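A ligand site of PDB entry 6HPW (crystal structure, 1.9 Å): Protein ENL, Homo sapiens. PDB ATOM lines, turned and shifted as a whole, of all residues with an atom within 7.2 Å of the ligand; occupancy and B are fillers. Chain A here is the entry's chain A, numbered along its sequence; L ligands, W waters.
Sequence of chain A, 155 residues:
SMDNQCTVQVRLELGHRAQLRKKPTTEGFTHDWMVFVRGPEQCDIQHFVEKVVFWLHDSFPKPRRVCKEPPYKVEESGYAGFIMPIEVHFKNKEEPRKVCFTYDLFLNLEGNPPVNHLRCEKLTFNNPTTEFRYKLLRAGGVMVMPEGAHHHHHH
Water W1 lies within hydrogen-bond range of the backbone carbonyl oxygen (O) of Ala 80 (2.8 Å), the indole nitrogen (NE1) of Trp 33 (2.9 Å) and an oxygen (O1) of the ligand (3.0 Å).
O1 of the ligand sits at hydrogen-bond distance from N of Tyr 79.
N1 of the ligand is in hydrogen-bond range of OG of Ser 59.
OH of Tyr 79 lies close to N1 of the ligand, 3.5 Å away.
The side-chain carboxylate of Glu 76 is in salt-bridge range of a nitrogen (N4) of the ligand (2.7 Å).
A nitrogen (N2) of the ligand is in hydrogen-bond range of the backbone carbonyl oxygen (O) of Ser 77.
The backbone NH (N) of Gly 78 sits at hydrogen-bond distance from the backbone carbonyl oxygen (O) of His 31 (2.9 Å).
The side-chain hydroxyl of Ser 59 lies within hydrogen-bond range of a ring nitrogen (ND1) of His 57 (2.8 Å).
The backbone NH (N) of Leu 105 sits at hydrogen-bond distance from the backbone carbonyl oxygen (O) of Phe 82, 2.9 Å away.
The guanidinium group (NH1) of Arg 65 lies within hydrogen-bond range of the backbone carbonyl oxygen (O) of Pro 61, 2.9 Å away.
The backbone NH of Trp 33 is in hydrogen-bond range of the backbone carbonyl oxygen of Glu 76 (2.8 Å).
The guanidinium group (NH1) of Arg 65 is in salt-bridge range of the side-chain carboxylate (OE2) of Glu 76 (2.9 Å).
Residues that only touch the ligand: Phe 29, His 57, Phe 60, Pro 61, Gly 78, Ala 80, Gly 81 and Phe 82.
The nearest printed residue that does not touch the ligand is Arg 65 (4.6 Å).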
ATOM      1  N   ARG A  21     -18.099  18.033  22.117  1.00  0.00           N
ATOM      2  CA  ARG A  21     -16.773  18.722  22.112  1.00  0.00           C
ATOM      3  C   ARG A  21     -15.850  17.868  22.945  1.00  0.00           C
ATOM      4  O   ARG A  21     -16.395  17.147  23.731  1.00  0.00           O
ATOM      5  CB  ARG A  21     -16.894  20.129  22.707  1.00  0.00           C
ATOM      6  CG  ARG A  21     -15.593  20.924  22.761  1.00  0.00           C
ATOM      7  CD  ARG A  21     -15.894  22.418  22.907  1.00  0.00           C
ATOM      8  NE  ARG A  21     -14.710  23.244  23.153  1.00  0.00           N
ATOM      9  CZ  ARG A  21     -13.949  23.834  22.210  1.00  0.00           C
ATOM     10  NH1 ARG A  21     -12.879  24.521  22.567  1.00  0.00           N
ATOM     11  NH2 ARG A  21     -14.224  23.686  20.913  1.00  0.00           N
ATOM     12  N   GLU A  27     -13.933  23.002  31.242  1.00  0.00           N
ATOM     13  CA  GLU A  27     -14.413  23.886  30.148  1.00  0.00           C
ATOM     14  C   GLU A  27     -15.869  23.474  29.863  1.00  0.00           C
ATOM     15  O   GLU A  27     -16.072  22.274  29.739  1.00  0.00           O
ATOM     16  CB  GLU A  27     -13.421  23.727  28.989  1.00  0.00           C
ATOM     17  CG  GLU A  27     -13.745  24.542  27.751  1.00  0.00           C
ATOM     18  CD  GLU A  27     -14.494  23.752  26.687  1.00  0.00           C
ATOM     19  OE1 GLU A  27     -15.123  22.716  27.063  1.00  0.00           O
ATOM     20  OE2 GLU A  27     -14.426  24.140  25.488  1.00  0.00           O
ATOM     21  N   PHE A  29     -18.444  24.026  27.639  1.00  0.00           N
ATOM     22  CA  PHE A  29     -19.110  23.829  26.322  1.00  0.00           C
ATOM     23  C   PHE A  29     -19.125  22.330  25.976  1.00  0.00           C
ATOM     24  O   PHE A  29     -18.007  21.688  25.840  1.00  0.00           O
ATOM     25  CB  PHE A  29     -18.386  24.645  25.269  1.00  0.00           C
ATOM     26  CG  PHE A  29     -18.200  26.097  25.660  1.00  0.00           C
ATOM     27  CD1 PHE A  29     -19.297  26.901  25.933  1.00  0.00           C
ATOM     28  CD2 PHE A  29     -16.944  26.658  25.699  1.00  0.00           C
ATOM     29  CE1 PHE A  29     -19.126  28.235  26.257  1.00  0.00           C
ATOM     30  CE2 PHE A  29     -16.772  27.980  26.094  1.00  0.00           C
ATOM     31  CZ  PHE A  29     -17.874  28.762  26.383  1.00  0.00           C
ATOM     32  N   HIS A  31     -20.513  21.028  23.260  1.00  0.00           N
ATOM     33  CA  HIS A  31     -20.715  20.811  21.801  1.00  0.00           C
ATOM     34  C   HIS A  31     -19.888  21.767  20.982  1.00  0.00           C
ATOM     35  O   HIS A  31     -19.674  22.897  21.399  1.00  0.00           O
ATOM     36  CB  HIS A  31     -22.202  20.945  21.426  1.00  0.00           C
ATOM     37  CG  HIS A  31     -23.043  19.787  21.818  1.00  0.00           C
ATOM     38  ND1 HIS A  31     -23.476  19.601  23.122  1.00  0.00           N
ATOM     39  CD2 HIS A  31     -23.557  18.774  21.092  1.00  0.00           C
ATOM     40  CE1 HIS A  31     -24.237  18.521  23.166  1.00  0.00           C
ATOM     41  NE2 HIS A  31     -24.304  17.999  21.939  1.00  0.00           N
ATOM     42  N   TRP A  33     -20.433  23.370  17.176  1.00  0.00           N
ATOM     43  CA  TRP A  33     -21.386  23.469  16.054  1.00  0.00           C
ATOM     44  C   TRP A  33     -20.890  24.434  14.999  1.00  0.00           C
ATOM     45  O   TRP A  33     -19.983  25.281  15.273  1.00  0.00           O
ATOM     46  CB  TRP A  33     -22.807  23.795  16.541  1.00  0.00           C
ATOM     47  CG  TRP A  33     -22.938  25.013  17.386  1.00  0.00           C
ATOM     48  CD1 TRP A  33     -23.125  25.079  18.748  1.00  0.00           C
ATOM     49  CD2 TRP A  33     -23.015  26.353  16.891  1.00  0.00           C
ATOM     50  NE1 TRP A  33     -23.316  26.382  19.134  1.00  0.00           N
ATOM     51  CE2 TRP A  33     -23.317  27.180  17.986  1.00  0.00           C
ATOM     52  CE3 TRP A  33     -22.986  26.910  15.590  1.00  0.00           C
ATOM     53  CZ2 TRP A  33     -23.474  28.567  17.836  1.00  0.00           C
ATOM     54  CZ3 TRP A  33     -23.080  28.273  15.466  1.00  0.00           C
ATOM     55  CH2 TRP A  33     -23.292  29.085  16.585  1.00  0.00           C
ATOM     56  N   HIS A  57     -27.366  33.410  20.222  1.00  0.00           N
ATOM     57  CA  HIS A  57     -27.912  33.589  21.573  1.00  0.00           C
ATOM     58  C   HIS A  57     -27.152  34.745  22.252  1.00  0.00           C
ATOM     59  O   HIS A  57     -25.885  34.811  22.085  1.00  0.00           O
ATOM     60  CB  HIS A  57     -27.854  32.276  22.337  1.00  0.00           C
ATOM     61  CG  HIS A  57     -28.617  32.351  23.607  1.00  0.00           C
ATOM     62  ND1 HIS A  57     -28.050  32.788  24.776  1.00  0.00           N
ATOM     63  CD2 HIS A  57     -29.946  32.239  23.835  1.00  0.00           C
ATOM     64  CE1 HIS A  57     -28.972  32.817  25.739  1.00  0.00           C
ATOM     65  NE2 HIS A  57     -30.157  32.490  25.170  1.00  0.00           N
ATOM     66  N   ASP A  58     -27.896  35.611  22.980  1.00  0.00           N
ATOM     67  CA  ASP A  58     -27.413  36.833  23.697  1.00  0.00           C
ATOM     68  C   ASP A  58     -26.251  36.487  24.626  1.00  0.00           C
ATOM     69  O   ASP A  58     -25.457  37.386  24.940  1.00  0.00           O
ATOM     70  CB  ASP A  58     -28.543  37.435  24.542  1.00  0.00           C
ATOM     71  CG  ASP A  58     -29.743  37.907  23.719  1.00  0.00           C
ATOM     72  OD1 ASP A  58     -29.518  38.389  22.651  1.00  0.00           O
ATOM     73  OD2 ASP A  58     -30.895  37.848  24.222  1.00  0.00           O
ATOM     74  N   SER A  59     -26.137  35.210  25.026  1.00  0.00           N
ATOM     75  CA  SER A  59     -25.084  34.729  25.953  1.00  0.00           C
ATOM     76  C   SER A  59     -23.716  34.710  25.242  1.00  0.00           C
ATOM     77  O   SER A  59     -22.698  34.732  25.925  1.00  0.00           O
ATOM     78  CB  SER A  59     -25.431  33.373  26.543  1.00  0.00           C
ATOM     79  OG  SER A  59     -25.416  32.360  25.545  1.00  0.00           O
ATOM     80  N   PHE A  60     -23.703  34.680  23.927  1.00  0.00           N
ATOM     81  CA  PHE A  60     -22.441  34.623  23.141  1.00  0.00           C
ATOM     82  C   PHE A  60     -21.792  36.001  23.140  1.00  0.00           C
ATOM     83  O   PHE A  60     -22.476  37.028  23.169  1.00  0.00           O
ATOM     84  CB  PHE A  60     -22.679  34.151  21.694  1.00  0.00           C
ATOM     85  CG  PHE A  60     -22.827  32.661  21.517  1.00  0.00           C
ATOM     86  CD1 PHE A  60     -24.056  32.048  21.669  1.00  0.00           C
ATOM     87  CD2 PHE A  60     -21.721  31.868  21.214  1.00  0.00           C
ATOM     88  CE1 PHE A  60     -24.189  30.669  21.525  1.00  0.00           C
ATOM     89  CE2 PHE A  60     -21.863  30.487  21.040  1.00  0.00           C
ATOM     90  CZ  PHE A  60     -23.088  29.890  21.225  1.00  0.00           C
ATOM     91  N   PRO A  61     -20.455  36.069  23.108  1.00  0.00           N
ATOM     92  CA  PRO A  61     -19.776  37.339  22.891  1.00  0.00           C
ATOM     93  C   PRO A  61     -19.965  37.727  21.411  1.00  0.00           C
ATOM     94  O   PRO A  61     -20.040  36.835  20.589  1.00  0.00           O
ATOM     95  CB  PRO A  61     -18.335  37.050  23.322  1.00  0.00           C
ATOM     96  CG  PRO A  61     -18.152  35.557  23.112  1.00  0.00           C
ATOM     97  CD  PRO A  61     -19.530  34.946  23.299  1.00  0.00           C
ATOM     98  N   ARG A  65     -22.929  38.132  14.237  1.00  0.00           N
ATOM     99  CA  ARG A  65     -21.781  37.600  13.467  1.00  0.00           C
ATOM    100  C   ARG A  65     -22.025  37.849  11.975  1.00  0.00           C
ATOM    101  O   ARG A  65     -23.034  37.372  11.437  1.00  0.00           O
ATOM    102  CB  ARG A  65     -21.613  36.103  13.725  1.00  0.00           C
ATOM    103  CG  ARG A  65     -21.352  35.761  15.184  1.00  0.00           C
ATOM    104  CD  ARG A  65     -20.053  36.286  15.706  1.00  0.00           C
ATOM    105  NE  ARG A  65     -19.905  35.951  17.112  1.00  0.00           N
ATOM    106  CZ  ARG A  65     -19.423  34.797  17.573  1.00  0.00           C
ATOM    107  NH1 ARG A  65     -19.380  34.586  18.878  1.00  0.00           N
ATOM    108  NH2 ARG A  65     -19.080  33.832  16.742  1.00  0.00           N
ATOM    109  N   GLU A  75     -18.579  29.146  13.252  1.00  0.00           N
ATOM    110  CA  GLU A  75     -18.087  27.951  13.952  1.00  0.00           C
ATOM    111  C   GLU A  75     -17.994  28.311  15.430  1.00  0.00           C
ATOM    112  O   GLU A  75     -17.321  29.294  15.740  1.00  0.00           O
ATOM    113  CB  GLU A  75     -16.735  27.504  13.376  1.00  0.00           C
ATOM    114  CG  GLU A  75     -16.893  26.890  12.008  1.00  0.00           C
ATOM    115  CD  GLU A  75     -15.618  26.788  11.180  1.00  0.00           C
ATOM    116  OE1 GLU A  75     -14.731  27.679  11.301  1.00  0.00           O
ATOM    117  OE2 GLU A  75     -15.561  25.865  10.351  1.00  0.00           O
ATOM    118  N   GLU A  76     -18.679  27.573  16.275  1.00  0.00           N
ATOM    119  CA  GLU A  76     -18.719  27.893  17.713  1.00  0.00           C
ATOM    120  C   GLU A  76     -18.664  26.627  18.550  1.00  0.00           C
ATOM    121  O   GLU A  76     -18.950  25.533  18.059  1.00  0.00           O
ATOM    122  CB  GLU A  76     -19.983  28.715  18.048  1.00  0.00           C
ATOM    123  CG  GLU A  76     -19.740  30.215  18.139  1.00  0.00           C
ATOM    124  CD  GLU A  76     -18.790  30.678  19.212  1.00  0.00           C
ATOM    125  OE1 GLU A  76     -18.372  29.834  20.086  1.00  0.00           O
ATOM    126  OE2 GLU A  76     -18.479  31.886  19.216  1.00  0.00           O
ATOM    127  N   SER A  77     -18.462  26.847  19.833  1.00  0.00           N
ATOM    128  CA  SER A  77     -18.687  25.889  20.919  1.00  0.00           C
ATOM    129  C   SER A  77     -19.891  26.360  21.756  1.00  0.00           C
ATOM    130  O   SER A  77     -20.151  27.592  21.785  1.00  0.00           O
ATOM    131  CB  SER A  77     -17.441  25.746  21.725  1.00  0.00           C
ATOM    132  OG  SER A  77     -17.081  26.997  22.353  1.00  0.00           O
ATOM    133  N   GLY A  78     -20.659  25.441  22.347  1.00  0.00           N
ATOM    134  CA  GLY A  78     -21.791  25.877  23.175  1.00  0.00           C
ATOM    135  C   GLY A  78     -22.355  24.785  24.026  1.00  0.00           C
ATOM    136  O   GLY A  78     -21.817  23.669  24.031  1.00  0.00           O
ATOM    137  N   TYR A  79     -23.368  25.112  24.811  1.00  0.00           N
ATOM    138  CA  TYR A  79     -23.918  24.152  25.783  1.00  0.00           C
ATOM    139  C   TYR A  79     -25.426  23.936  25.560  1.00  0.00           C
ATOM    140  O   TYR A  79     -25.956  23.132  26.252  1.00  0.00           O
ATOM    141  CB  TYR A  79     -23.576  24.562  27.221  1.00  0.00           C
ATOM    142  CG  TYR A  79     -23.787  26.017  27.561  1.00  0.00           C
ATOM    143  CD1 TYR A  79     -25.070  26.529  27.767  1.00  0.00           C
ATOM    144  CD2 TYR A  79     -22.718  26.883  27.772  1.00  0.00           C
ATOM    145  CE1 TYR A  79     -25.269  27.842  28.188  1.00  0.00           C
ATOM    146  CE2 TYR A  79     -22.899  28.219  28.133  1.00  0.00           C
ATOM    147  CZ  TYR A  79     -24.190  28.711  28.346  1.00  0.00           C
ATOM    148  OH  TYR A  79     -24.405  30.049  28.578  1.00  0.00           O
ATOM    149  N   ALA A  80     -26.056  24.589  24.563  1.00  0.00           N
ATOM    150  CA  ALA A  80     -27.491  24.434  24.291  1.00  0.00           C
ATOM    151  C   ALA A  80     -27.810  24.903  22.860  1.00  0.00           C
ATOM    152  O   ALA A  80     -27.105  25.778  22.322  1.00  0.00           O
ATOM    153  CB  ALA A  80     -28.280  25.199  25.325  1.00  0.00           C
ATOM    154  N   GLY A  81     -28.865  24.340  22.300  1.00  0.00           N
ATOM    155  CA  GLY A  81     -29.473  24.792  21.047  1.00  0.00           C
ATOM    156  C   GLY A  81     -30.239  26.069  21.270  1.00  0.00           C
ATOM    157  O   GLY A  81     -30.554  26.377  22.416  1.00  0.00           O
ATOM    158  N   PHE A  82     -30.569  26.772  20.205  1.00  0.00           N
ATOM    159  CA  PHE A  82     -31.390  27.998  20.269  1.00  0.00           C
ATOM    160  C   PHE A  82     -31.889  28.282  18.867  1.00  0.00           C
ATOM    161  O   PHE A  82     -31.423  27.636  17.901  1.00  0.00           O
ATOM    162  CB  PHE A  82     -30.591  29.186  20.824  1.00  0.00           C
ATOM    163  CG  PHE A  82     -29.297  29.454  20.107  1.00  0.00           C
ATOM    164  CD1 PHE A  82     -28.172  28.664  20.341  1.00  0.00           C
ATOM    165  CD2 PHE A  82     -29.195  30.438  19.109  1.00  0.00           C
ATOM    166  CE1 PHE A  82     -26.998  28.867  19.628  1.00  0.00           C
ATOM    167  CE2 PHE A  82     -28.024  30.610  18.390  1.00  0.00           C
ATOM    168  CZ  PHE A  82     -26.915  29.853  18.685  1.00  0.00           C
ATOM    169  N   ILE A  83     -32.793  29.208  18.795  1.00  0.00           N
ATOM    170  CA  ILE A  83     -33.362  29.741  17.553  1.00  0.00           C
ATOM    171  C   ILE A  83     -32.478  30.903  17.144  1.00  0.00           C
ATOM    172  O   ILE A  83     -32.272  31.830  17.974  1.00  0.00           O
ATOM    173  CB  ILE A  83     -34.809  30.150  17.793  1.00  0.00           C
ATOM    174  CG1 ILE A  83     -35.664  28.952  18.200  1.00  0.00           C
ATOM    175  CG2 ILE A  83     -35.361  30.829  16.572  1.00  0.00           C
ATOM    176  CD1 ILE A  83     -35.504  27.770  17.317  1.00  0.00           C
ATOM    177  N   LEU A 105     -31.149  25.943  15.557  1.00  0.00           N
ATOM    178  CA  LEU A 105     -29.810  25.409  15.855  1.00  0.00           C
ATOM    179  C   LEU A 105     -29.908  24.452  17.035  1.00  0.00           C
ATOM    180  O   LEU A 105     -29.653  24.893  18.173  1.00  0.00           O
ATOM    181  CB  LEU A 105     -28.820  26.530  16.136  1.00  0.00           C
ATOM    182  CG  LEU A 105     -27.397  26.095  15.852  1.00  0.00           C
ATOM    183  CD1 LEU A 105     -26.646  27.149  15.088  1.00  0.00           C
ATOM    184  CD2 LEU A 105     -26.678  25.683  17.066  1.00  0.00           C
ATOM    185  N   LEU A 107     -28.815  20.807  19.028  1.00  0.00           N
ATOM    186  CA  LEU A 107     -27.618  19.974  19.313  1.00  0.00           C
ATOM    187  C   LEU A 107     -28.019  18.492  19.407  1.00  0.00           C
ATOM    188  O   LEU A 107     -29.199  18.239  19.632  1.00  0.00           O
ATOM    189  CB  LEU A 107     -27.008  20.449  20.619  1.00  0.00           C
ATOM    190  CG  LEU A 107     -26.593  21.918  20.645  1.00  0.00           C
ATOM    191  CD1 LEU A 107     -25.877  22.226  21.959  1.00  0.00           C
ATOM    192  CD2 LEU A 107     -25.740  22.282  19.460  1.00  0.00           C
HETATM  193  C1  LIG L   1     -28.818  28.909  25.323  1.00  0.00           C
HETATM  194  C2  LIG L   1     -28.197  28.439  24.163  1.00  0.00           C
HETATM  195  C3  LIG L   1     -26.831  28.538  23.968  1.00  0.00           C
HETATM  196  C4  LIG L   1     -26.025  29.123  24.925  1.00  0.00           C
HETATM  197  C5  LIG L   1     -26.623  29.616  26.086  1.00  0.00           C
HETATM  198  C6  LIG L   1     -27.990  29.481  26.294  1.00  0.00           C
HETATM  199  C7  LIG L   1     -24.550  29.110  24.738  1.00  0.00           C
HETATM  200  O1  LIG L   1     -23.986  28.144  24.233  1.00  0.00           O
HETATM  201  I1  LIG L   1     -28.770  29.918  28.239  1.00  0.00           I
HETATM  202  C8  LIG L   1     -30.316  28.829  25.451  1.00  0.00           C
HETATM  203  N1  LIG L   1     -23.897  30.212  25.151  1.00  0.00           N
HETATM  204  C9  LIG L   1     -22.522  30.488  25.025  1.00  0.00           C
HETATM  205  C10 LIG L   1     -21.699  29.735  24.184  1.00  0.00           C
HETATM  206  C11 LIG L   1     -20.381  30.138  24.002  1.00  0.00           C
HETATM  207  C12 LIG L   1     -19.910  31.259  24.677  1.00  0.00           C
HETATM  208  C13 LIG L   1     -20.704  31.996  25.530  1.00  0.00           C
HETATM  209  C14 LIG L   1     -22.018  31.604  25.704  1.00  0.00           C
HETATM  210  N2  LIG L   1     -19.375  29.600  23.222  1.00  0.00           N
HETATM  211  C15 LIG L   1     -18.325  30.374  23.436  1.00  0.00           C
HETATM  212  N3  LIG L   1     -18.593  31.389  24.289  1.00  0.00           N
HETATM  213  C16 LIG L   1     -16.952  30.125  22.891  1.00  0.00           C
HETATM  214  N4  LIG L   1     -16.633  30.978  21.746  1.00  0.00           N
HETATM  215  C17 LIG L   1     -15.341  30.563  21.145  1.00  0.00           C
HETATM  216  C18 LIG L   1     -15.039  31.308  19.864  1.00  0.00           C
HETATM  217  C19 LIG L   1     -15.307  32.797  20.014  1.00  0.00           C
HETATM  218  C20 LIG L   1     -15.431  33.166  21.476  1.00  0.00           C
HETATM  219  C21 LIG L   1     -16.562  32.395  22.147  1.00  0.00           C
HETATM  220  O   HOH W   1     -24.581  26.808  21.663  1.00  0.00           O
